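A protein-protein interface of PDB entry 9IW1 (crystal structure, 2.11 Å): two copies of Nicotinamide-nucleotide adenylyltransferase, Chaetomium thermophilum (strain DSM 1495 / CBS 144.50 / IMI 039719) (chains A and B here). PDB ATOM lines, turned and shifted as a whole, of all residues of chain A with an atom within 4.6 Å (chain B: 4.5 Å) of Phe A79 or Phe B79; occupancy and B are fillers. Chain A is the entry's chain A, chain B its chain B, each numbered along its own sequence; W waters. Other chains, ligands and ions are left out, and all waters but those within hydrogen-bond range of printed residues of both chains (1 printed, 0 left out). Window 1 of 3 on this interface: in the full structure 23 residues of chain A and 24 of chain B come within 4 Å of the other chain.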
ATOM      1  N   THR A  78     -36.776  13.707 -11.487  1.00  0.00           N
ATOM      2  CA  THR A  78     -35.621  14.606 -11.556  1.00  0.00           C
ATOM      3  C   THR A  78     -34.350  13.823 -11.863  1.00  0.00           C
ATOM      4  O   THR A  78     -34.321  12.590 -11.817  1.00  0.00           O
ATOM      5  CB  THR A  78     -35.400  15.381 -10.250  1.00  0.00           C
ATOM      6  OG1 THR A  78     -34.676  14.562  -9.330  1.00  0.00           O
ATOM      7  CG2 THR A  78     -36.716  15.777  -9.601  1.00  0.00           C
ATOM      8  N   PHE A  79     -33.271  14.562 -12.145  1.00  0.00           N
ATOM      9  CA  PHE A  79     -31.982  13.916 -12.358  1.00  0.00           C
ATOM     10  C   PHE A  79     -31.486  13.215 -11.095  1.00  0.00           C
ATOM     11  O   PHE A  79     -30.739  12.235 -11.188  1.00  0.00           O
ATOM     12  CB  PHE A  79     -30.957  14.936 -12.838  1.00  0.00           C
ATOM     13  CG  PHE A  79     -30.984  15.172 -14.328  1.00  0.00           C
ATOM     14  CD1 PHE A  79     -30.926  14.111 -15.215  1.00  0.00           C
ATOM     15  CD2 PHE A  79     -31.086  16.461 -14.836  1.00  0.00           C
ATOM     16  CE1 PHE A  79     -30.944  14.322 -16.590  1.00  0.00           C
ATOM     17  CE2 PHE A  79     -31.111  16.682 -16.211  1.00  0.00           C
ATOM     18  CZ  PHE A  79     -31.037  15.612 -17.088  1.00  0.00           C
ATOM     19  N   LEU A  80     -31.894  13.685  -9.913  1.00  0.00           N
ATOM     20  CA  LEU A  80     -31.493  13.014  -8.679  1.00  0.00           C
ATOM     21  C   LEU A  80     -32.100  11.617  -8.588  1.00  0.00           C
ATOM     22  O   LEU A  80     -31.413  10.653  -8.232  1.00  0.00           O
ATOM     23  CB  LEU A  80     -31.905  13.837  -7.463  1.00  0.00           C
ATOM     24  CG  LEU A  80     -31.493  13.206  -6.124  1.00  0.00           C
ATOM     25  CD1 LEU A  80     -30.002  12.866  -6.121  1.00  0.00           C
ATOM     26  CD2 LEU A  80     -31.808  14.128  -4.971  1.00  0.00           C
ATOM     27  N   HIS A  81     -33.395  11.488  -8.893  1.00  0.00           N
ATOM     28  CA  HIS A  81     -34.018  10.169  -8.911  1.00  0.00           C
ATOM     29  C   HIS A  81     -33.252   9.228  -9.825  1.00  0.00           C
ATOM     30  O   HIS A  81     -33.015   8.067  -9.477  1.00  0.00           O
ATOM     31  CB  HIS A  81     -35.473  10.267  -9.384  1.00  0.00           C
ATOM     32  CG  HIS A  81     -36.370  11.062  -8.483  1.00  0.00           C
ATOM     33  ND1 HIS A  81     -37.188  12.067  -8.951  1.00  0.00           N
ATOM     34  CD2 HIS A  81     -36.613  10.973  -7.153  1.00  0.00           C
ATOM     35  CE1 HIS A  81     -37.875  12.584  -7.947  1.00  0.00           C
ATOM     36  NE2 HIS A  81     -37.547  11.934  -6.845  1.00  0.00           N
ATOM     37  N   LEU A  82     -32.837   9.718 -10.996  1.00  0.00           N
ATOM     38  CA  LEU A  82     -32.116   8.863 -11.933  1.00  0.00           C
ATOM     39  C   LEU A  82     -30.717   8.551 -11.425  1.00  0.00           C
ATOM     40  O   LEU A  82     -30.254   7.408 -11.527  1.00  0.00           O
ATOM     41  CB  LEU A  82     -32.051   9.528 -13.311  1.00  0.00           C
ATOM     42  CG  LEU A  82     -33.413   9.686 -13.998  1.00  0.00           C
ATOM     43  CD1 LEU A  82     -33.328  10.578 -15.232  1.00  0.00           C
ATOM     44  CD2 LEU A  82     -33.966   8.325 -14.372  1.00  0.00           C
ATOM     45  N   ARG A  83     -30.041   9.547 -10.851  1.00  0.00           N
ATOM     46  CA  ARG A  83     -28.696   9.338 -10.328  1.00  0.00           C
ATOM     47  C   ARG A  83     -28.671   8.287  -9.222  1.00  0.00           C
ATOM     48  O   ARG A  83     -27.688   7.550  -9.096  1.00  0.00           O
ATOM     49  CB  ARG A  83     -28.125  10.676  -9.846  1.00  0.00           C
ATOM     50  CG  ARG A  83     -26.688  10.619  -9.353  1.00  0.00           C
ATOM     51  CD  ARG A  83     -25.755  10.113 -10.421  1.00  0.00           C
ATOM     52  NE  ARG A  83     -24.449   9.791  -9.859  1.00  0.00           N
ATOM     53  CZ  ARG A  83     -23.511   9.103 -10.499  1.00  0.00           C
ATOM     54  NH1 ARG A  83     -23.667   8.725 -11.761  1.00  0.00           N
ATOM     55  NH2 ARG A  83     -22.395   8.777  -9.854  1.00  0.00           N
ATOM     56  N   TYR A 272     -31.726  21.399 -16.769  1.00  0.00           N
ATOM     57  CA  TYR A 272     -30.583  20.767 -16.108  1.00  0.00           C
ATOM     58  C   TYR A 272     -30.879  20.319 -14.680  1.00  0.00           C
ATOM     59  O   TYR A 272     -29.966  19.840 -14.006  1.00  0.00           O
ATOM     60  CB  TYR A 272     -29.346  21.677 -16.120  1.00  0.00           C
ATOM     61  CG  TYR A 272     -29.146  22.252 -17.498  1.00  0.00           C
ATOM     62  CD1 TYR A 272     -28.960  21.409 -18.588  1.00  0.00           C
ATOM     63  CD2 TYR A 272     -29.191  23.616 -17.724  1.00  0.00           C
ATOM     64  CE1 TYR A 272     -28.800  21.903 -19.864  1.00  0.00           C
ATOM     65  CE2 TYR A 272     -29.028  24.137 -19.001  1.00  0.00           C
ATOM     66  CZ  TYR A 272     -28.826  23.267 -20.069  1.00  0.00           C
ATOM     67  OH  TYR A 272     -28.668  23.748 -21.349  1.00  0.00           O
ATOM     68  N   LEU A 273     -32.116  20.457 -14.197  1.00  0.00           N
ATOM     69  CA  LEU A 273     -32.562  19.811 -12.967  1.00  0.00           C
ATOM     70  C   LEU A 273     -33.343  18.541 -13.237  1.00  0.00           C
ATOM     71  O   LEU A 273     -33.355  17.631 -12.401  1.00  0.00           O
ATOM     72  CB  LEU A 273     -33.450  20.756 -12.151  1.00  0.00           C
ATOM     73  CG  LEU A 273     -32.836  22.078 -11.701  1.00  0.00           C
ATOM     74  CD1 LEU A 273     -33.881  22.907 -10.941  1.00  0.00           C
ATOM     75  CD2 LEU A 273     -31.577  21.850 -10.855  1.00  0.00           C
ATOM     76  N   ILE A 274     -34.017  18.494 -14.380  1.00  0.00           N
ATOM     77  CA  ILE A 274     -34.763  17.334 -14.854  1.00  0.00           C
ATOM     78  C   ILE A 274     -34.476  17.170 -16.338  1.00  0.00           C
ATOM     79  O   ILE A 274     -33.997  18.105 -16.996  1.00  0.00           O
ATOM     80  CB  ILE A 274     -36.280  17.493 -14.612  1.00  0.00           C
ATOM     81  CG1 ILE A 274     -36.887  18.481 -15.608  1.00  0.00           C
ATOM     82  CG2 ILE A 274     -36.541  17.958 -13.178  1.00  0.00           C
ATOM     83  CD1 ILE A 274     -38.330  18.877 -15.252  1.00  0.00           C
ATOM     84  N   PRO A 275     -34.732  15.982 -16.893  1.00  0.00           N
ATOM     85  CA  PRO A 275     -34.337  15.722 -18.282  1.00  0.00           C
ATOM     86  C   PRO A 275     -35.071  16.614 -19.276  1.00  0.00           C
ATOM     87  O   PRO A 275     -36.235  16.965 -19.078  1.00  0.00           O
ATOM     88  CB  PRO A 275     -34.699  14.243 -18.482  1.00  0.00           C
ATOM     89  CG  PRO A 275     -34.673  13.663 -17.103  1.00  0.00           C
ATOM     90  CD  PRO A 275     -35.225  14.758 -16.232  1.00  0.00           C
ATOM     91  N   THR B  78     -20.171  19.800 -16.917  1.00  0.00           N
ATOM     92  CA  THR B  78     -21.122  19.062 -16.095  1.00  0.00           C
ATOM     93  C   THR B  78     -22.478  19.764 -16.101  1.00  0.00           C
ATOM     94  O   THR B  78     -22.641  20.864 -16.645  1.00  0.00           O
ATOM     95  CB  THR B  78     -20.629  18.929 -14.656  1.00  0.00           C
ATOM     96  OG1 THR B  78     -20.792  20.181 -13.986  1.00  0.00           O
ATOM     97  CG2 THR B  78     -19.155  18.542 -14.630  1.00  0.00           C
ATOM     98  N   PHE B  79     -23.461  19.106 -15.479  1.00  0.00           N
ATOM     99  CA  PHE B  79     -24.773  19.722 -15.308  1.00  0.00           C
ATOM    100  C   PHE B  79     -24.702  20.965 -14.435  1.00  0.00           C
ATOM    101  O   PHE B  79     -25.528  21.867 -14.572  1.00  0.00           O
ATOM    102  CB  PHE B  79     -25.751  18.721 -14.695  1.00  0.00           C
ATOM    103  CG  PHE B  79     -26.366  17.805 -15.696  1.00  0.00           C
ATOM    104  CD1 PHE B  79     -26.752  18.279 -16.935  1.00  0.00           C
ATOM    105  CD2 PHE B  79     -26.540  16.464 -15.413  1.00  0.00           C
ATOM    106  CE1 PHE B  79     -27.315  17.435 -17.878  1.00  0.00           C
ATOM    107  CE2 PHE B  79     -27.100  15.616 -16.349  1.00  0.00           C
ATOM    108  CZ  PHE B  79     -27.490  16.106 -17.585  1.00  0.00           C
ATOM    109  N   LEU B  80     -23.736  21.036 -13.535  1.00  0.00           N
ATOM    110  CA  LEU B  80     -23.614  22.223 -12.702  1.00  0.00           C
ATOM    111  C   LEU B  80     -23.208  23.447 -13.525  1.00  0.00           C
ATOM    112  O   LEU B  80     -23.742  24.542 -13.313  1.00  0.00           O
ATOM    113  CB  LEU B  80     -22.626  21.947 -11.569  1.00  0.00           C
ATOM    114  CG  LEU B  80     -22.450  22.964 -10.433  1.00  0.00           C
ATOM    115  CD1 LEU B  80     -21.356  23.955 -10.753  1.00  0.00           C
ATOM    116  CD2 LEU B  80     -23.765  23.684 -10.138  1.00  0.00           C
ATOM    117  N   HIS B  81     -22.244  23.290 -14.445  1.00  0.00           N
ATOM    118  CA  HIS B  81     -21.860  24.401 -15.321  1.00  0.00           C
ATOM    119  C   HIS B  81     -23.057  24.935 -16.085  1.00  0.00           C
ATOM    120  O   HIS B  81     -23.194  26.149 -16.278  1.00  0.00           O
ATOM    121  CB  HIS B  81     -20.770  23.960 -16.301  1.00  0.00           C
ATOM    122  CG  HIS B  81     -19.490  23.563 -15.636  1.00  0.00           C
ATOM    123  ND1 HIS B  81     -18.741  22.486 -16.052  1.00  0.00           N
ATOM    124  CD2 HIS B  81     -18.839  24.088 -14.570  1.00  0.00           C
ATOM    125  CE1 HIS B  81     -17.674  22.369 -15.279  1.00  0.00           C
ATOM    126  NE2 HIS B  81     -17.711  23.328 -14.371  1.00  0.00           N
ATOM    127  N   LEU B  82     -23.911  24.035 -16.570  1.00  0.00           N
ATOM    128  CA  LEU B  82     -25.079  24.449 -17.331  1.00  0.00           C
ATOM    129  C   LEU B  82     -26.111  25.091 -16.421  1.00  0.00           C
ATOM    130  O   LEU B  82     -26.703  26.115 -16.776  1.00  0.00           O
ATOM    131  CB  LEU B  82     -25.662  23.249 -18.075  1.00  0.00           C
ATOM    132  CG  LEU B  82     -24.667  22.661 -19.075  1.00  0.00           C
ATOM    133  CD1 LEU B  82     -25.009  21.220 -19.412  1.00  0.00           C
ATOM    134  CD2 LEU B  82     -24.621  23.525 -20.331  1.00  0.00           C
ATOM    135  N   ARG B  83     -26.306  24.525 -15.224  1.00  0.00           N
ATOM    136  CA  ARG B  83     -27.247  25.097 -14.267  1.00  0.00           C
ATOM    137  C   ARG B  83     -26.864  26.529 -13.913  1.00  0.00           C
ATOM    138  O   ARG B  83     -27.733  27.362 -13.631  1.00  0.00           O
ATOM    139  CB  ARG B  83     -27.297  24.242 -12.999  1.00  0.00           C
ATOM    140  CG  ARG B  83     -28.545  23.412 -12.813  1.00  0.00           C
ATOM    141  CD  ARG B  83     -29.806  24.163 -13.203  1.00  0.00           C
ATOM    142  NE  ARG B  83     -30.377  24.960 -12.122  1.00  0.00           N
ATOM    143  CZ  ARG B  83     -31.562  25.548 -12.193  1.00  0.00           C
ATOM    144  NH1 ARG B  83     -32.340  25.406 -13.257  1.00  0.00           N
ATOM    145  NH2 ARG B  83     -31.980  26.293 -11.173  1.00  0.00           N
ATOM    146  N   TYR B 272     -26.089  11.096 -15.505  1.00  0.00           N
ATOM    147  CA  TYR B 272     -26.918  12.035 -14.741  1.00  0.00           C
ATOM    148  C   TYR B 272     -26.091  13.024 -13.925  1.00  0.00           C
ATOM    149  O   TYR B 272     -26.663  13.857 -13.212  1.00  0.00           O
ATOM    150  CB  TYR B 272     -27.931  11.314 -13.836  1.00  0.00           C
ATOM    151  CG  TYR B 272     -28.677  10.258 -14.615  1.00  0.00           C
ATOM    152  CD1 TYR B 272     -29.468  10.611 -15.687  1.00  0.00           C
ATOM    153  CD2 TYR B 272     -28.556   8.910 -14.304  1.00  0.00           C
ATOM    154  CE1 TYR B 272     -30.141   9.660 -16.431  1.00  0.00           C
ATOM    155  CE2 TYR B 272     -29.221   7.948 -15.040  1.00  0.00           C
ATOM    156  CZ  TYR B 272     -30.015   8.332 -16.105  1.00  0.00           C
ATOM    157  OH  TYR B 272     -30.685   7.395 -16.856  1.00  0.00           O
ATOM    158  N   LEU B 273     -24.768  12.988 -14.027  1.00  0.00           N
ATOM    159  CA  LEU B 273     -23.941  14.081 -13.539  1.00  0.00           C
ATOM    160  C   LEU B 273     -23.517  15.027 -14.658  1.00  0.00           C
ATOM    161  O   LEU B 273     -23.287  16.213 -14.409  1.00  0.00           O
ATOM    162  CB  LEU B 273     -22.694  13.529 -12.839  1.00  0.00           C
ATOM    163  CG  LEU B 273     -22.882  12.623 -11.615  1.00  0.00           C
ATOM    164  CD1 LEU B 273     -21.511  12.178 -11.092  1.00  0.00           C
ATOM    165  CD2 LEU B 273     -23.668  13.329 -10.524  1.00  0.00           C
ATOM    166  N   ILE B 274     -23.401  14.509 -15.873  1.00  0.00           N
ATOM    167  CA  ILE B 274     -23.063  15.278 -17.069  1.00  0.00           C
ATOM    168  C   ILE B 274     -23.983  14.804 -18.176  1.00  0.00           C
ATOM    169  O   ILE B 274     -24.593  13.730 -18.063  1.00  0.00           O
ATOM    170  CB  ILE B 274     -21.583  15.085 -17.470  1.00  0.00           C
ATOM    171  CG1 ILE B 274     -21.363  13.696 -18.048  1.00  0.00           C
ATOM    172  CG2 ILE B 274     -20.647  15.281 -16.270  1.00  0.00           C
ATOM    173  CD1 ILE B 274     -19.894  13.356 -18.318  1.00  0.00           C
ATOM    174  N   PRO B 275     -24.154  15.593 -19.238  1.00  0.00           N
ATOM    175  CA  PRO B 275     -25.146  15.227 -20.256  1.00  0.00           C
ATOM    176  C   PRO B 275     -24.786  13.932 -20.970  1.00  0.00           C
ATOM    177  O   PRO B 275     -23.615  13.645 -21.222  1.00  0.00           O
ATOM    178  CB  PRO B 275     -25.129  16.418 -21.219  1.00  0.00           C
ATOM    179  CG  PRO B 275     -24.604  17.548 -20.404  1.00  0.00           C
ATOM    180  CD  PRO B 275     -23.619  16.952 -19.463  1.00  0.00           C
HETATM  181  O   HOH W   1     -27.946  14.206 -10.676  1.00  0.00           O
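Among the printed residues, pairs that only touch across the chains: Phe A79 with Phe B79 (3.6 Å), Phe A79 with Tyr B272 (3.8 Å), Leu A82 with Tyr B272 (3.5 Å), Arg A83 with Tyr B272 (3.8 Å), Arg A83 with Leu B273 (3.7 Å), Tyr A272 with Leu B82 (3.6 Å), Tyr A272 with Arg B83 (3.8 Å) and Leu A273 with Arg B83 (3.6 Å).
Phe B79 touches its own counterpart, Phe A79.
Phe A79 touches Tyr B272, but with the chains exchanged Tyr A272 does not touch Phe B79 (4.1 Å).
Arg A83 touches Tyr B272, and with the chains exchanged Tyr A272 touches Arg B83.
Arg A83 touches Leu B273, and with the chains exchanged Leu A273 touches Arg B83.
The backbone NH (N) of Phe A79 sits at hydrogen-bond distance from the backbone carbonyl oxygen (O) of Leu A273 (3.1 Å).
The backbone NH of Phe B79 lies within hydrogen-bond range of the backbone carbonyl oxygen of Leu B273, at 3.1 Å.
Water W1 lies within hydrogen-bond range of O of Tyr B272 (2.9 Å) and O of Phe A79 (3.5 Å).
Phe A79 touches two residues of chain B.
Of the printed residues of chain A, Leu B82 touches Tyr A272 (3.6 Å).
Of the printed residues of chain A, Arg B83 touches Tyr A272 (3.8 Å) and Leu A273 (3.6 Å).
Ile B274 touches none of the printed residues of chain A.
The nearest printed residue of chain B that does not touch Phe A79 is Leu B273 (6.4 Å).
The nearest residue of chain A that does not touch Phe B79 is Tyr A272 (4.1 Å).
Hydrophobic or aromatic side chains of chain A within 4 Å of the printed part of chain B: Phe A79, Leu A82, Tyr A272 and Leu A273.
Hydrophobic or aromatic side chains of chain B within 4 Å of the printed part of chain A: Phe B79, Leu B82, Tyr B272 and Leu B273.
Among the printed residues, 8 pairs touch across the chains.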
